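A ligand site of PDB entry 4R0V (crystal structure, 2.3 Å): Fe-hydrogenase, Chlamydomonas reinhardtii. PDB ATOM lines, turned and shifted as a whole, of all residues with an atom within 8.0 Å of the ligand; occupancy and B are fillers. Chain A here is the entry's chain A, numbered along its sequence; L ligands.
Merely in contact with the ligand: Pro 171 (3.8 Å), Ala 416 (3.8 Å), Gly 420 (3.8 Å) and Gly 424 (3.9 Å).
Hydrophobic or aromatic side chains within 4 Å of the ligand: Pro 171 and Ala 416.
Of the 30 residues printed, 8 come within 4 Å of the ligand.
N of Cys 421 sits close to S4 of the ligand, at 3.5 Å.
SG of Cys 421 is bound to FE2 of the ligand (2.2 Å).
SG of Cys 417 is bound to FE1 of the ligand, at 2.3 Å.
SG of Cys 225 binds FE4 of the ligand (2.4 Å).
SG of Cys 170 binds FE3 of the ligand, 2.4 Å away.
OD1 of Asn 390 sits close to O of Cys 417 (3.1 Å).
SG of Cys 225 sits close to N of Lys 228 (3.8 Å).
N of Arg 227 sits close to SG of Cys 225 (3.4 Å).
The side-chain sulfur (SG) of Cys 170 lies close to the backbone NH (N) of Ala 416 (3.4 Å).
The side-chain sulfur (SG) of Cys 170 lies close to the backbone NH (N) of Gly 172, 3.4 Å away.
SG of Cys 170 lies close to N of Trp 173 (3.8 Å).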
ATOM      1  N   ALA A  94      18.785   1.061 -13.152  1.00  0.00           N
ATOM      2  CA  ALA A  94      17.484   0.498 -12.766  1.00  0.00           C
ATOM      3  C   ALA A  94      17.116  -0.693 -13.637  1.00  0.00           C
ATOM      4  O   ALA A  94      16.384  -1.550 -13.214  1.00  0.00           O
ATOM      5  CB  ALA A  94      16.400   1.575 -12.819  1.00  0.00           C
ATOM      6  N   CSO A 169      16.084  15.797 -15.505  1.00  0.00           N
ATOM      7  CA  CSO A 169      16.420  14.490 -16.056  1.00  0.00           C
ATOM      8  CB  CSO A 169      17.458  13.749 -15.164  1.00  0.00           C
ATOM      9  SG  CSO A 169      16.811  13.614 -13.508  1.00  0.00           S
ATOM     10  C   CSO A 169      15.144  13.688 -16.354  1.00  0.00           C
ATOM     11  O   CSO A 169      15.185  12.731 -17.144  1.00  0.00           O
ATOM     12  OD  CSO A 169      18.261  13.117 -12.544  1.00  0.00           O
ATOM     13  N   CYS A 170      14.006  14.034 -15.744  1.00  0.00           N
ATOM     14  CA  CYS A 170      12.773  13.282 -16.013  1.00  0.00           C
ATOM     15  C   CYS A 170      11.950  13.870 -17.146  1.00  0.00           C
ATOM     16  O   CYS A 170      11.512  15.023 -17.037  1.00  0.00           O
ATOM     17  CB  CYS A 170      11.887  13.180 -14.731  1.00  0.00           C
ATOM     18  SG  CYS A 170      10.381  12.164 -14.986  1.00  0.00           S
ATOM     19  N   PRO A 171      11.653  13.063 -18.228  1.00  0.00           N
ATOM     20  CA  PRO A 171      10.928  13.652 -19.365  1.00  0.00           C
ATOM     21  C   PRO A 171       9.506  13.868 -19.011  1.00  0.00           C
ATOM     22  O   PRO A 171       8.841  14.641 -19.678  1.00  0.00           O
ATOM     23  CB  PRO A 171      11.040  12.632 -20.494  1.00  0.00           C
ATOM     24  CG  PRO A 171      11.948  11.516 -20.027  1.00  0.00           C
ATOM     25  CD  PRO A 171      12.293  11.767 -18.572  1.00  0.00           C
ATOM     26  N   GLY A 172       9.030  13.205 -17.965  1.00  0.00           N
ATOM     27  CA  GLY A 172       7.638  13.331 -17.580  1.00  0.00           C
ATOM     28  C   GLY A 172       7.442  14.669 -16.973  1.00  0.00           C
ATOM     29  O   GLY A 172       6.436  15.300 -17.187  1.00  0.00           O
ATOM     30  N   TRP A 173       8.429  15.130 -16.215  1.00  0.00           N
ATOM     31  CA  TRP A 173       8.365  16.480 -15.642  1.00  0.00           C
ATOM     32  C   TRP A 173       8.507  17.530 -16.747  1.00  0.00           C
ATOM     33  O   TRP A 173       7.786  18.511 -16.765  1.00  0.00           O
ATOM     34  CB  TRP A 173       9.403  16.626 -14.548  1.00  0.00           C
ATOM     35  CG  TRP A 173       9.936  17.989 -14.286  1.00  0.00           C
ATOM     36  CD1 TRP A 173      11.255  18.326 -14.335  1.00  0.00           C
ATOM     37  CD2 TRP A 173       9.219  19.184 -13.964  1.00  0.00           C
ATOM     38  NE1 TRP A 173      11.393  19.654 -14.026  1.00  0.00           N
ATOM     39  CE2 TRP A 173      10.170  20.204 -13.801  1.00  0.00           C
ATOM     40  CE3 TRP A 173       7.868  19.505 -13.848  1.00  0.00           C
ATOM     41  CZ2 TRP A 173       9.836  21.505 -13.497  1.00  0.00           C
ATOM     42  CZ3 TRP A 173       7.518  20.786 -13.529  1.00  0.00           C
ATOM     43  CH2 TRP A 173       8.497  21.796 -13.356  1.00  0.00           C
ATOM     44  N   MET A 223      16.347   1.394 -20.884  1.00  0.00           N
ATOM     45  CA  MET A 223      15.831   2.271 -19.843  1.00  0.00           C
ATOM     46  C   MET A 223      14.664   1.684 -19.146  1.00  0.00           C
ATOM     47  O   MET A 223      13.939   0.904 -19.720  1.00  0.00           O
ATOM     48  CB  MET A 223      15.389   3.586 -20.486  1.00  0.00           C
ATOM     49  CG  MET A 223      16.556   4.438 -20.919  1.00  0.00           C
ATOM     50  SD  MET A 223      17.383   5.317 -19.549  1.00  0.00           S
ATOM     51  CE  MET A 223      19.049   4.967 -20.078  1.00  0.00           C
ATOM     52  N   PRO A 224      14.395   2.131 -17.909  1.00  0.00           N
ATOM     53  CA  PRO A 224      13.275   1.584 -17.139  1.00  0.00           C
ATOM     54  C   PRO A 224      11.983   2.302 -17.422  1.00  0.00           C
ATOM     55  O   PRO A 224      10.985   2.088 -16.747  1.00  0.00           O
ATOM     56  CB  PRO A 224      13.690   1.836 -15.698  1.00  0.00           C
ATOM     57  CG  PRO A 224      14.476   3.088 -15.801  1.00  0.00           C
ATOM     58  CD  PRO A 224      15.168   3.088 -17.108  1.00  0.00           C
ATOM     59  N   CYS A 225      11.990   3.090 -18.479  1.00  0.00           N
ATOM     60  CA  CYS A 225      11.047   4.150 -18.615  1.00  0.00           C
ATOM     61  C   CYS A 225      10.464   4.195 -20.019  1.00  0.00           C
ATOM     62  O   CYS A 225      11.185   4.050 -21.017  1.00  0.00           O
ATOM     63  CB  CYS A 225      11.858   5.406 -18.320  1.00  0.00           C
ATOM     64  SG  CYS A 225      11.031   6.960 -18.594  1.00  0.00           S
ATOM     65  N   THR A 226       9.167   4.419 -20.089  1.00  0.00           N
ATOM     66  CA  THR A 226       8.426   4.490 -21.340  1.00  0.00           C
ATOM     67  C   THR A 226       8.511   5.892 -22.008  1.00  0.00           C
ATOM     68  O   THR A 226       8.126   6.065 -23.126  1.00  0.00           O
ATOM     69  CB  THR A 226       6.932   4.196 -21.068  1.00  0.00           C
ATOM     70  OG1 THR A 226       6.488   4.983 -19.936  1.00  0.00           O
ATOM     71  CG2 THR A 226       6.727   2.748 -20.718  1.00  0.00           C
ATOM     72  N   ARG A 227       9.016   6.877 -21.291  1.00  0.00           N
ATOM     73  CA  ARG A 227       9.118   8.247 -21.814  1.00  0.00           C
ATOM     74  C   ARG A 227      10.468   8.694 -22.376  1.00  0.00           C
ATOM     75  O   ARG A 227      10.572   9.804 -22.871  1.00  0.00           O
ATOM     76  CB  ARG A 227       8.721   9.205 -20.724  1.00  0.00           C
ATOM     77  CG  ARG A 227       7.364   8.858 -20.119  1.00  0.00           C
ATOM     78  CD  ARG A 227       7.061   9.989 -19.161  1.00  0.00           C
ATOM     79  NE  ARG A 227       6.190   9.630 -18.072  1.00  0.00           N
ATOM     80  CZ  ARG A 227       5.057  10.250 -17.778  1.00  0.00           C
ATOM     81  NH1 ARG A 227       4.628  11.297 -18.529  1.00  0.00           N
ATOM     82  NH2 ARG A 227       4.364   9.834 -16.706  1.00  0.00           N
ATOM     83  N   LYS A 228      11.469   7.855 -22.254  1.00  0.00           N
ATOM     84  CA  LYS A 228      12.824   8.198 -22.581  1.00  0.00           C
ATOM     85  C   LYS A 228      12.987   8.214 -24.076  1.00  0.00           C
ATOM     86  O   LYS A 228      13.877   8.873 -24.537  1.00  0.00           O
ATOM     87  CB  LYS A 228      13.838   7.240 -21.950  1.00  0.00           C
ATOM     88  CG  LYS A 228      14.075   7.539 -20.440  1.00  0.00           C
ATOM     89  CD  LYS A 228      14.976   8.728 -20.261  1.00  0.00           C
ATOM     90  CE  LYS A 228      15.130   9.206 -18.790  1.00  0.00           C
ATOM     91  NZ  LYS A 228      15.944  10.479 -18.881  1.00  0.00           N
ATOM     92  N   GLU A 231      12.119  11.738 -24.981  1.00  0.00           N
ATOM     93  CA  GLU A 231      13.268  12.598 -24.689  1.00  0.00           C
ATOM     94  C   GLU A 231      14.252  12.549 -25.838  1.00  0.00           C
ATOM     95  O   GLU A 231      14.650  13.583 -26.368  1.00  0.00           O
ATOM     96  CB  GLU A 231      13.948  12.186 -23.416  1.00  0.00           C
ATOM     97  CG  GLU A 231      15.188  12.976 -23.003  1.00  0.00           C
ATOM     98  CD  GLU A 231      15.819  12.344 -21.765  1.00  0.00           C
ATOM     99  OE1 GLU A 231      15.382  12.590 -20.642  1.00  0.00           O
ATOM    100  OE2 GLU A 231      16.714  11.507 -21.890  1.00  0.00           O
ATOM    101  N   ASN A 390       7.901  13.346  -5.872  1.00  0.00           N
ATOM    102  CA  ASN A 390       7.406  12.171  -6.611  1.00  0.00           C
ATOM    103  C   ASN A 390       5.872  12.059  -6.459  1.00  0.00           C
ATOM    104  O   ASN A 390       5.417  11.965  -5.339  1.00  0.00           O
ATOM    105  CB  ASN A 390       7.988  10.888  -5.997  1.00  0.00           C
ATOM    106  CG  ASN A 390       9.503  10.779  -6.097  1.00  0.00           C
ATOM    107  OD1 ASN A 390      10.033  10.292  -7.070  1.00  0.00           O
ATOM    108  ND2 ASN A 390      10.198  11.171  -5.038  1.00  0.00           N
ATOM    109  N   GLY A 391       5.064  12.015  -7.512  1.00  0.00           N
ATOM    110  CA  GLY A 391       5.473  12.233  -8.895  1.00  0.00           C
ATOM    111  C   GLY A 391       4.953  13.526  -9.505  1.00  0.00           C
ATOM    112  O   GLY A 391       5.503  14.590  -9.253  1.00  0.00           O
ATOM    113  N   LEU A 392       3.902  13.436 -10.323  1.00  0.00           N
ATOM    114  CA  LEU A 392       3.411  14.621 -11.031  1.00  0.00           C
ATOM    115  C   LEU A 392       2.261  15.365 -10.342  1.00  0.00           C
ATOM    116  O   LEU A 392       2.262  16.585 -10.283  1.00  0.00           O
ATOM    117  CB  LEU A 392       3.007  14.259 -12.469  1.00  0.00           C
ATOM    118  CG  LEU A 392       4.155  13.929 -13.430  1.00  0.00           C
ATOM    119  CD1 LEU A 392       3.681  13.966 -14.866  1.00  0.00           C
ATOM    120  CD2 LEU A 392       5.322  14.871 -13.215  1.00  0.00           C
ATOM    121  N   ILE A 414      11.999  17.036  -9.417  1.00  0.00           N
ATOM    122  CA  ILE A 414      10.708  16.424  -9.707  1.00  0.00           C
ATOM    123  C   ILE A 414      10.871  15.139 -10.530  1.00  0.00           C
ATOM    124  O   ILE A 414      11.479  15.215 -11.600  1.00  0.00           O
ATOM    125  CB  ILE A 414       9.876  17.456 -10.446  1.00  0.00           C
ATOM    126  CG1 ILE A 414       9.534  18.626  -9.470  1.00  0.00           C
ATOM    127  CG2 ILE A 414       8.606  16.777 -10.922  1.00  0.00           C
ATOM    128  CD1 ILE A 414       8.742  19.736 -10.095  1.00  0.00           C
ATOM    129  N   MET A 415      10.412  13.985 -10.005  1.00  0.00           N
ATOM    130  CA  MET A 415      10.315  12.746 -10.824  1.00  0.00           C
ATOM    131  C   MET A 415       8.832  12.360 -11.012  1.00  0.00           C
ATOM    132  O   MET A 415       8.038  12.445 -10.099  1.00  0.00           O
ATOM    133  CB  MET A 415      11.132  11.577 -10.233  1.00  0.00           C
ATOM    134  CG  MET A 415      12.607  11.841  -9.889  1.00  0.00           C
ATOM    135  SD  MET A 415      13.786  12.108 -11.234  1.00  0.00           S
ATOM    136  CE  MET A 415      15.363  11.795 -10.430  1.00  0.00           C
ATOM    137  N   ALA A 416       8.452  11.935 -12.216  1.00  0.00           N
ATOM    138  CA  ALA A 416       7.028  11.581 -12.499  1.00  0.00           C
ATOM    139  C   ALA A 416       6.488  10.273 -11.849  1.00  0.00           C
ATOM    140  O   ALA A 416       5.255  10.163 -11.588  1.00  0.00           O
ATOM    141  CB  ALA A 416       6.801  11.512 -14.012  1.00  0.00           C
ATOM    142  N   CYS A 417       7.372   9.300 -11.593  1.00  0.00           N
ATOM    143  CA  CYS A 417       7.051   8.026 -10.983  1.00  0.00           C
ATOM    144  C   CYS A 417       7.103   8.152  -9.464  1.00  0.00           C
ATOM    145  O   CYS A 417       8.082   8.676  -8.903  1.00  0.00           O
ATOM    146  CB  CYS A 417       7.993   6.925 -11.440  1.00  0.00           C
ATOM    147  SG  CYS A 417       7.823   6.592 -13.226  1.00  0.00           S
ATOM    148  N   PRO A 418       6.034   7.647  -8.770  1.00  0.00           N
ATOM    149  CA  PRO A 418       5.994   7.623  -7.290  1.00  0.00           C
ATOM    150  C   PRO A 418       7.229   7.037  -6.596  1.00  0.00           C
ATOM    151  O   PRO A 418       7.618   7.555  -5.527  1.00  0.00           O
ATOM    152  CB  PRO A 418       4.736   6.781  -6.979  1.00  0.00           C
ATOM    153  CG  PRO A 418       3.798   7.128  -8.119  1.00  0.00           C
ATOM    154  CD  PRO A 418       4.742   7.190  -9.357  1.00  0.00           C
ATOM    155  N   ALA A 419       7.871   5.995  -7.192  1.00  0.00           N
ATOM    156  CA  ALA A 419       9.118   5.412  -6.612  1.00  0.00           C
ATOM    157  C   ALA A 419      10.455   5.721  -7.355  1.00  0.00           C
ATOM    158  O   ALA A 419      11.520   5.169  -7.019  1.00  0.00           O
ATOM    159  CB  ALA A 419       8.943   3.906  -6.444  1.00  0.00           C
ATOM    160  N   GLY A 420      10.406   6.646  -8.302  1.00  0.00           N
ATOM    161  CA  GLY A 420      11.537   6.944  -9.148  1.00  0.00           C
ATOM    162  C   GLY A 420      11.742   5.843 -10.188  1.00  0.00           C
ATOM    163  O   GLY A 420      10.934   4.976 -10.387  1.00  0.00           O
ATOM    164  N   CYS A 421      12.860   5.908 -10.861  1.00  0.00           N
ATOM    165  CA  CYS A 421      13.149   5.100 -11.980  1.00  0.00           C
ATOM    166  C   CYS A 421      13.079   3.614 -11.673  1.00  0.00           C
ATOM    167  O   CYS A 421      12.671   2.882 -12.529  1.00  0.00           O
ATOM    168  CB  CYS A 421      14.473   5.537 -12.585  1.00  0.00           C
ATOM    169  SG  CYS A 421      14.435   7.305 -13.112  1.00  0.00           S
ATOM    170  N   VAL A 422      13.417   3.149 -10.484  1.00  0.00           N
ATOM    171  CA  VAL A 422      13.238   1.751 -10.175  1.00  0.00           C
ATOM    172  C   VAL A 422      11.836   1.286 -10.323  1.00  0.00           C
ATOM    173  O   VAL A 422      11.640   0.106 -10.512  1.00  0.00           O
ATOM    174  CB  VAL A 422      13.756   1.295  -8.763  1.00  0.00           C
ATOM    175  CG1 VAL A 422      15.268   1.434  -8.751  1.00  0.00           C
ATOM    176  CG2 VAL A 422      13.157   2.089  -7.596  1.00  0.00           C
ATOM    177  N   GLY A 423      10.870   2.202 -10.235  1.00  0.00           N
ATOM    178  CA  GLY A 423       9.458   1.937 -10.468  1.00  0.00           C
ATOM    179  C   GLY A 423       8.868   2.441 -11.779  1.00  0.00           C
ATOM    180  O   GLY A 423       7.656   2.587 -11.903  1.00  0.00           O
ATOM    181  N   GLY A 424       9.728   2.698 -12.756  1.00  0.00           N
ATOM    182  CA  GLY A 424       9.330   3.104 -14.089  1.00  0.00           C
ATOM    183  C   GLY A 424       8.341   2.193 -14.782  1.00  0.00           C
ATOM    184  O   GLY A 424       8.198   0.955 -14.456  1.00  0.00           O
ATOM    185  N   GLY A 425       7.683   2.770 -15.763  1.00  0.00           N
ATOM    186  CA  GLY A 425       6.618   2.056 -16.374  1.00  0.00           C
ATOM    187  C   GLY A 425       7.141   0.988 -17.319  1.00  0.00           C
ATOM    188  O   GLY A 425       6.347   0.216 -17.855  1.00  0.00           O
ATOM    189  N   GLY A 426       8.438   1.009 -17.577  1.00  0.00           N
ATOM    190  CA  GLY A 426       9.103   0.001 -18.422  1.00  0.00           C
ATOM    191  C   GLY A 426       9.646  -1.205 -17.629  1.00  0.00           C
ATOM    192  O   GLY A 426      10.223  -2.138 -18.226  1.00  0.00           O
ATOM    193  N   GLN A 427       9.471  -1.159 -16.298  1.00  0.00           N
ATOM    194  CA  GLN A 427       9.885  -2.248 -15.425  1.00  0.00           C
ATOM    195  C   GLN A 427       8.912  -3.421 -15.395  1.00  0.00           C
ATOM    196  O   GLN A 427       7.682  -3.283 -15.634  1.00  0.00           O
ATOM    197  CB  GLN A 427      10.094  -1.738 -13.985  1.00  0.00           C
ATOM    198  CG  GLN A 427      11.141  -0.656 -13.902  1.00  0.00           C
ATOM    199  CD  GLN A 427      12.547  -1.155 -14.074  1.00  0.00           C
ATOM    200  OE1 GLN A 427      12.917  -1.734 -15.102  1.00  0.00           O
ATOM    201  NE2 GLN A 427      13.330  -0.931 -13.070  1.00  0.00           N
HETATM  202 FE1  LIG L   1       9.950   7.317 -13.689  1.00  0.00          FE
HETATM  203 FE2  LIG L   1      12.845   7.499 -14.612  1.00  0.00          FE
HETATM  204 FE3  LIG L   1      11.130  10.032 -14.292  1.00  0.00          FE
HETATM  205 FE4  LIG L   1      10.576   8.041 -16.546  1.00  0.00          FE
HETATM  206  S1  LIG L   1      12.279   9.142 -15.867  1.00  0.00           S
HETATM  207  S2  LIG L   1       9.414   8.951 -14.965  1.00  0.00           S
HETATM  208  S3  LIG L   1      11.114   6.427 -15.247  1.00  0.00           S
HETATM  209  S4  LIG L   1      11.687   8.379 -13.040  1.00  0.00           S
